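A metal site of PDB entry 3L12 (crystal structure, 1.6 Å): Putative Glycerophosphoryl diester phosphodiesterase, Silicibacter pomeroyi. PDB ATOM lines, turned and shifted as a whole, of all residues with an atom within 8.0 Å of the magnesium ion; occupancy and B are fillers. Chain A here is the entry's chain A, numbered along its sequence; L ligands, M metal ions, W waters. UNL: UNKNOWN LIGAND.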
ATOM      1  N   HIS A  23     -24.296  32.644  16.791  1.00  0.00           N
ATOM      2  CA  HIS A  23     -23.770  31.330  16.387  1.00  0.00           C
ATOM      3  C   HIS A  23     -24.126  31.020  14.919  1.00  0.00           C
ATOM      4  O   HIS A  23     -25.323  30.889  14.558  1.00  0.00           O
ATOM      5  CB  HIS A  23     -24.312  30.253  17.311  1.00  0.00           C
ATOM      6  CG  HIS A  23     -23.620  28.941  17.149  1.00  0.00           C
ATOM      7  ND1 HIS A  23     -24.323  27.767  16.921  1.00  0.00           N
ATOM      8  CD2 HIS A  23     -22.315  28.611  17.157  1.00  0.00           C
ATOM      9  CE1 HIS A  23     -23.441  26.762  16.853  1.00  0.00           C
ATOM     10  NE2 HIS A  23     -22.225  27.260  16.971  1.00  0.00           N
ATOM     11  N   ARG A  24     -23.096  30.919  14.063  1.00  0.00           N
ATOM     12  CA  ARG A  24     -23.235  30.737  12.602  1.00  0.00           C
ATOM     13  C   ARG A  24     -24.118  31.831  12.022  1.00  0.00           C
ATOM     14  O   ARG A  24     -24.761  31.648  11.064  1.00  0.00           O
ATOM     15  CB  ARG A  24     -23.784  29.332  12.262  1.00  0.00           C
ATOM     16  CG  ARG A  24     -23.026  28.265  13.008  1.00  0.00           C
ATOM     17  CD  ARG A  24     -23.495  26.871  12.685  1.00  0.00           C
ATOM     18  NE  ARG A  24     -22.751  25.967  13.532  1.00  0.00           N
ATOM     19  CZ  ARG A  24     -22.980  24.657  13.662  1.00  0.00           C
ATOM     20  NH1 ARG A  24     -23.943  24.028  12.960  1.00  0.00           N
ATOM     21  NH2 ARG A  24     -22.269  23.959  14.555  1.00  0.00           N
ATOM     22  N   ASN A  33     -24.641  29.859   8.695  1.00  0.00           N
ATOM     23  CA  ASN A  33     -23.458  30.083   7.879  1.00  0.00           C
ATOM     24  C   ASN A  33     -23.754  30.583   6.445  1.00  0.00           C
ATOM     25  O   ASN A  33     -23.046  30.240   5.439  1.00  0.00           O
ATOM     26  CB  ASN A  33     -22.570  28.837   7.918  1.00  0.00           C
ATOM     27  CG  ASN A  33     -21.780  28.730   9.185  1.00  0.00           C
ATOM     28  OD1 ASN A  33     -21.359  29.744   9.749  1.00  0.00           O
ATOM     29  ND2 ASN A  33     -21.483  27.487   9.619  1.00  0.00           N
ATOM     30  N   GLU A  50     -19.914  34.245  15.183  1.00  0.00           N
ATOM     31  CA  GLU A  50     -19.111  33.058  15.114  1.00  0.00           C
ATOM     32  C   GLU A  50     -19.488  32.302  13.846  1.00  0.00           C
ATOM     33  O   GLU A  50     -20.668  32.252  13.451  1.00  0.00           O
ATOM     34  CB  GLU A  50     -19.341  32.202  16.311  1.00  0.00           C
ATOM     35  CG  GLU A  50     -18.457  30.961  16.439  1.00  0.00           C
ATOM     36  CD  GLU A  50     -18.947  29.698  15.726  1.00  0.00           C
ATOM     37  OE1 GLU A  50     -20.033  29.689  15.151  1.00  0.00           O
ATOM     38  OE2 GLU A  50     -18.234  28.641  15.764  1.00  0.00           O
ATOM     39  N   PHE A  51     -18.504  31.715  13.198  1.00  0.00           N
ATOM     40  CA  PHE A  51     -18.743  30.947  12.019  1.00  0.00           C
ATOM     41  C   PHE A  51     -17.561  29.978  11.832  1.00  0.00           C
ATOM     42  O   PHE A  51     -16.545  30.111  12.509  1.00  0.00           O
ATOM     43  CB  PHE A  51     -18.914  31.859  10.826  1.00  0.00           C
ATOM     44  CG  PHE A  51     -17.740  32.758  10.603  1.00  0.00           C
ATOM     45  CD1 PHE A  51     -17.662  33.967  11.243  1.00  0.00           C
ATOM     46  CD2 PHE A  51     -16.683  32.371   9.757  1.00  0.00           C
ATOM     47  CE1 PHE A  51     -16.571  34.820  11.033  1.00  0.00           C
ATOM     48  CE2 PHE A  51     -15.581  33.213   9.552  1.00  0.00           C
ATOM     49  CZ  PHE A  51     -15.558  34.460  10.192  1.00  0.00           C
ATOM     50  N   ASP A  52     -17.706  29.060  10.874  1.00  0.00           N
ATOM     51  CA  ASP A  52     -16.775  27.948  10.734  1.00  0.00           C
ATOM     52  C   ASP A  52     -16.159  27.989   9.364  1.00  0.00           C
ATOM     53  O   ASP A  52     -16.874  28.361   8.392  1.00  0.00           O
ATOM     54  CB  ASP A  52     -17.495  26.632  10.917  1.00  0.00           C
ATOM     55  CG  ASP A  52     -18.390  26.653  12.149  1.00  0.00           C
ATOM     56  OD1 ASP A  52     -17.829  26.535  13.286  1.00  0.00           O
ATOM     57  OD2 ASP A  52     -19.632  26.794  11.958  1.00  0.00           O
ATOM     58  N   VAL A  53     -14.890  27.577   9.277  1.00  0.00           N
ATOM     59  CA  VAL A  53     -14.199  27.552   8.002  1.00  0.00           C
ATOM     60  C   VAL A  53     -13.565  26.193   7.784  1.00  0.00           C
ATOM     61  O   VAL A  53     -12.944  25.641   8.671  1.00  0.00           O
ATOM     62  CB  VAL A  53     -13.146  28.665   7.892  1.00  0.00           C
ATOM     63  CG1 VAL A  53     -12.377  28.618   6.534  1.00  0.00           C
ATOM     64  CG2 VAL A  53     -13.823  30.041   8.112  1.00  0.00           C
ATOM     65  N   THR A  64     -18.821  26.705   6.349  1.00  0.00           N
ATOM     66  CA  THR A  64     -19.732  25.577   6.610  1.00  0.00           C
ATOM     67  C   THR A  64     -19.235  24.930   7.896  1.00  0.00           C
ATOM     68  O   THR A  64     -18.029  24.943   8.154  1.00  0.00           O
ATOM     69  CB  THR A  64     -19.867  24.621   5.407  1.00  0.00           C
ATOM     70  OG1 THR A  64     -20.887  23.658   5.715  1.00  0.00           O
ATOM     71  CG2 THR A  64     -18.617  23.929   5.098  1.00  0.00           C
ATOM     72  N   HIS A  65     -20.152  24.325   8.645  1.00  0.00           N
ATOM     73  CA  HIS A  65     -19.852  23.912  10.006  1.00  0.00           C
ATOM     74  C   HIS A  65     -19.037  22.678  10.177  1.00  0.00           C
ATOM     75  O   HIS A  65     -18.416  22.517  11.224  1.00  0.00           O
ATOM     76  CB  HIS A  65     -21.144  23.765  10.844  1.00  0.00           C
ATOM     77  CG  HIS A  65     -21.809  22.421  10.717  1.00  0.00           C
ATOM     78  ND1 HIS A  65     -22.559  22.057   9.621  1.00  0.00           N
ATOM     79  CD2 HIS A  65     -21.823  21.358  11.554  1.00  0.00           C
ATOM     80  CE1 HIS A  65     -22.986  20.813   9.778  1.00  0.00           C
ATOM     81  NE2 HIS A  65     -22.596  20.395  10.964  1.00  0.00           N
ATOM     82  N   ASN A  66     -19.077  21.786   9.184  1.00  0.00           N
ATOM     83  CA  ASN A  66     -18.330  20.550   9.243  1.00  0.00           C
ATOM     84  C   ASN A  66     -17.583  20.162   7.965  1.00  0.00           C
ATOM     85  O   ASN A  66     -17.817  20.671   6.885  1.00  0.00           O
ATOM     86  CB  ASN A  66     -19.307  19.437   9.605  1.00  0.00           C
ATOM     87  CG  ASN A  66     -18.624  18.213  10.110  1.00  0.00           C
ATOM     88  OD1 ASN A  66     -17.516  18.293  10.701  1.00  0.00           O
ATOM     89  ND2 ASN A  66     -19.221  17.049   9.831  1.00  0.00           N
ATOM     90  N   LEU A 147     -15.337  35.506  15.511  1.00  0.00           N
ATOM     91  CA  LEU A 147     -14.813  34.339  16.178  1.00  0.00           C
ATOM     92  C   LEU A 147     -14.803  33.304  15.045  1.00  0.00           C
ATOM     93  O   LEU A 147     -15.813  32.665  14.714  1.00  0.00           O
ATOM     94  CB  LEU A 147     -15.770  33.997  17.301  1.00  0.00           C
ATOM     95  CG  LEU A 147     -15.345  33.119  18.424  1.00  0.00           C
ATOM     96  CD1 LEU A 147     -14.037  33.673  19.153  1.00  0.00           C
ATOM     97  CD2 LEU A 147     -16.487  32.970  19.407  1.00  0.00           C
ATOM     98  N   LEU A 148     -13.636  33.180  14.403  1.00  0.00           N
ATOM     99  CA  LEU A 148     -13.457  32.375  13.204  1.00  0.00           C
ATOM    100  C   LEU A 148     -13.002  30.983  13.612  1.00  0.00           C
ATOM    101  O   LEU A 148     -11.855  30.755  14.039  1.00  0.00           O
ATOM    102  CB  LEU A 148     -12.475  33.090  12.286  1.00  0.00           C
ATOM    103  CG  LEU A 148     -12.250  32.545  10.895  1.00  0.00           C
ATOM    104  CD1 LEU A 148     -11.540  33.631  10.096  1.00  0.00           C
ATOM    105  CD2 LEU A 148     -11.494  31.196  10.862  1.00  0.00           C
ATOM    106  N   GLU A 149     -13.937  30.047  13.542  1.00  0.00           N
ATOM    107  CA  GLU A 149     -13.653  28.661  13.972  1.00  0.00           C
ATOM    108  C   GLU A 149     -12.983  27.910  12.815  1.00  0.00           C
ATOM    109  O   GLU A 149     -13.628  27.626  11.783  1.00  0.00           O
ATOM    110  CB  GLU A 149     -14.891  27.910  14.448  1.00  0.00           C
ATOM    111  CG  GLU A 149     -14.490  26.606  15.127  1.00  0.00           C
ATOM    112  CD  GLU A 149     -15.608  25.693  15.576  1.00  0.00           C
ATOM    113  OE1 GLU A 149     -16.739  26.124  15.808  1.00  0.00           O
ATOM    114  OE2 GLU A 149     -15.287  24.464  15.774  1.00  0.00           O
ATOM    115  N   LEU A 150     -11.707  27.573  12.986  1.00  0.00           N
ATOM    116  CA  LEU A 150     -11.024  26.728  12.027  1.00  0.00           C
ATOM    117  C   LEU A 150     -11.415  25.273  12.333  1.00  0.00           C
ATOM    118  O   LEU A 150     -11.164  24.805  13.449  1.00  0.00           O
ATOM    119  CB  LEU A 150      -9.531  26.888  12.160  1.00  0.00           C
ATOM    120  CG  LEU A 150      -8.966  28.241  11.673  1.00  0.00           C
ATOM    121  CD1 LEU A 150      -8.920  29.175  12.856  1.00  0.00           C
ATOM    122  CD2 LEU A 150      -7.595  28.110  11.048  1.00  0.00           C
ATOM    123  N   LYS A 151     -12.039  24.611  11.351  1.00  0.00           N
ATOM    124  CA  LYS A 151     -12.562  23.225  11.461  1.00  0.00           C
ATOM    125  C   LYS A 151     -11.660  22.374  10.594  1.00  0.00           C
ATOM    126  O   LYS A 151     -11.754  22.344   9.353  1.00  0.00           O
ATOM    127  CB  LYS A 151     -14.043  23.143  11.043  1.00  0.00           C
ATOM    128  CG  LYS A 151     -14.743  21.794  11.309  1.00  0.00           C
ATOM    129  CD  LYS A 151     -15.017  21.676  12.814  1.00  0.00           C
ATOM    130  CE  LYS A 151     -16.076  20.652  13.178  1.00  0.00           C
ATOM    131  NZ  LYS A 151     -15.428  19.338  13.423  1.00  0.00           N
ATOM    132  N   HIS A 186     -10.024  30.682  16.353  1.00  0.00           N
ATOM    133  CA  HIS A 186     -10.813  29.895  17.305  1.00  0.00           C
ATOM    134  C   HIS A 186     -10.887  28.442  16.880  1.00  0.00           C
ATOM    135  O   HIS A 186     -11.120  28.185  15.703  1.00  0.00           O
ATOM    136  CB  HIS A 186     -12.177  30.615  17.313  1.00  0.00           C
ATOM    137  CG  HIS A 186     -13.283  30.026  18.133  1.00  0.00           C
ATOM    138  ND1 HIS A 186     -13.337  30.104  19.509  1.00  0.00           N
ATOM    139  CD2 HIS A 186     -14.472  29.496  17.737  1.00  0.00           C
ATOM    140  CE1 HIS A 186     -14.487  29.583  19.927  1.00  0.00           C
ATOM    141  NE2 HIS A 186     -15.194  29.217  18.869  1.00  0.00           N
ATOM    142  N   PHE A 188     -11.248  23.935  18.223  1.00  0.00           N
ATOM    143  CA  PHE A 188     -11.086  22.759  19.058  1.00  0.00           C
ATOM    144  C   PHE A 188      -9.692  22.173  18.842  1.00  0.00           C
ATOM    145  O   PHE A 188      -9.213  21.436  19.669  1.00  0.00           O
ATOM    146  CB  PHE A 188     -12.086  21.648  18.739  1.00  0.00           C
ATOM    147  CG  PHE A 188     -13.425  21.798  19.433  1.00  0.00           C
ATOM    148  CD1 PHE A 188     -13.581  21.453  20.755  1.00  0.00           C
ATOM    149  CD2 PHE A 188     -14.505  22.233  18.714  1.00  0.00           C
ATOM    150  CE1 PHE A 188     -14.856  21.528  21.356  1.00  0.00           C
ATOM    151  CE2 PHE A 188     -15.761  22.330  19.344  1.00  0.00           C
ATOM    152  CZ  PHE A 188     -15.906  21.966  20.636  1.00  0.00           C
ATOM    153  N   LEU A 208     -11.584  26.262  22.262  1.00  0.00           N
ATOM    154  CA  LEU A 208     -12.825  25.587  22.530  1.00  0.00           C
ATOM    155  C   LEU A 208     -12.545  24.369  23.389  1.00  0.00           C
ATOM    156  O   LEU A 208     -11.516  23.656  23.206  1.00  0.00           O
ATOM    157  CB  LEU A 208     -13.469  25.082  21.222  1.00  0.00           C
ATOM    158  CG  LEU A 208     -14.133  26.187  20.437  1.00  0.00           C
ATOM    159  CD1 LEU A 208     -14.375  25.845  18.943  1.00  0.00           C
ATOM    160  CD2 LEU A 208     -15.478  26.463  21.140  1.00  0.00           C
ATOM    161  N   TRP A 274     -20.792  28.620  25.009  1.00  0.00           N
ATOM    162  CA  TRP A 274     -21.547  28.244  23.810  1.00  0.00           C
ATOM    163  C   TRP A 274     -22.214  26.911  23.992  1.00  0.00           C
ATOM    164  O   TRP A 274     -21.842  26.219  24.970  1.00  0.00           O
ATOM    165  CB  TRP A 274     -20.587  28.109  22.579  1.00  0.00           C
ATOM    166  CG  TRP A 274     -19.561  27.055  22.789  1.00  0.00           C
ATOM    167  CD1 TRP A 274     -18.377  27.204  23.442  1.00  0.00           C
ATOM    168  CD2 TRP A 274     -19.642  25.681  22.408  1.00  0.00           C
ATOM    169  NE1 TRP A 274     -17.733  25.992  23.522  1.00  0.00           N
ATOM    170  CE2 TRP A 274     -18.478  25.035  22.899  1.00  0.00           C
ATOM    171  CE3 TRP A 274     -20.616  24.908  21.734  1.00  0.00           C
ATOM    172  CZ2 TRP A 274     -18.230  23.692  22.678  1.00  0.00           C
ATOM    173  CZ3 TRP A 274     -20.355  23.556  21.540  1.00  0.00           C
ATOM    174  CH2 TRP A 274     -19.170  22.974  22.013  1.00  0.00           C
ATOM    175  N   THR A 275     -23.297  26.567  23.258  1.00  0.00           N
ATOM    176  CA  THR A 275     -24.154  27.412  22.421  1.00  0.00           C
ATOM    177  C   THR A 275     -25.409  27.473  23.319  1.00  0.00           C
ATOM    178  O   THR A 275     -26.049  26.453  23.593  1.00  0.00           O
ATOM    179  CB  THR A 275     -24.447  26.829  21.073  1.00  0.00           C
ATOM    180  OG1 THR A 275     -23.233  26.830  20.303  1.00  0.00           O
ATOM    181  CG2 THR A 275     -25.499  27.613  20.386  1.00  0.00           C
ATOM    182  N   VAL A 294     -22.372  32.745  23.178  1.00  0.00           N
ATOM    183  CA  VAL A 294     -22.601  32.368  21.821  1.00  0.00           C
ATOM    184  C   VAL A 294     -23.955  31.662  21.828  1.00  0.00           C
ATOM    185  O   VAL A 294     -24.169  30.682  22.548  1.00  0.00           O
ATOM    186  CB  VAL A 294     -21.500  31.399  21.307  1.00  0.00           C
ATOM    187  CG1 VAL A 294     -21.751  30.992  19.864  1.00  0.00           C
ATOM    188  CG2 VAL A 294     -20.120  32.061  21.464  1.00  0.00           C
HETATM  189  O1  UNL L   1     -18.953  23.898  18.019  1.00  0.00           O
HETATM  190  O2  UNL L   1     -18.293  25.068  18.684  1.00  0.00           O
HETATM  191  O3  UNL L   1     -19.350  26.203  18.457  1.00  0.00           O
HETATM  192  O4  UNL L   1     -19.662  26.557  17.105  1.00  0.00           O
HETATM  193  O5  UNL L   1     -18.811  27.634  19.015  1.00  0.00           O
HETATM  194  O6  UNL L   1     -17.651  28.038  18.363  1.00  0.00           O
HETATM  195 MG    MG M   1     -18.537  26.627  15.221  1.00  0.00          MG
HETATM  196  O   HOH W   1     -20.384  27.178  14.432  1.00  0.00           O
HETATM  197  O   HOH W   2     -19.132  24.579  15.101  1.00  0.00           O
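Water W1 lies within hydrogen-bond range of OD2 of Asp 52 (2.6 Å), OE1 of Glu 50 (2.6 Å), NE of Arg 24 (2.8 Å) and NE2 of His 23 (3.1 Å).
The side-chain carboxylate (OD2) of Asp 52 is in salt-bridge range of the guanidinium group (NE) of Arg 24.
The backbone carbonyl oxygen (O) of Asp 52 is in hydrogen-bond range of the backbone NH (N) of Thr 64.
OD2 of Asp 52 sits at hydrogen-bond distance from ND2 of Asn 33, at 3.1 Å.
N of Val 53 sits at hydrogen-bond distance from O of Glu 149 (2.8 Å).
The backbone NH (N) of Arg 24 is in hydrogen-bond range of the backbone carbonyl oxygen (O) of Glu 50, 2.8 Å away.
The backbone NH (N) of Glu 149 sits at hydrogen-bond distance from the backbone carbonyl oxygen (O) of Phe 51, at 2.8 Å.
Within 4 Å of the magnesium ion: Glu 50, Asp 52 and Glu 149.
Along chain A the residues within 4 Å of the magnesium ion span positions 50 to 149.
The magnesium ion is bound by the side-chain carboxylate (OE1) of Glu 149 (2.0 Å), the side-chain carboxylate (OD1) of Asp 52 (2.1 Å), water W1 (2.1 Å), the side-chain carboxylate (OE2) of Glu 50 (2.1 Å), water W2 (2.1 Å) and an oxygen (O4) of the ligand (2.2 Å).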
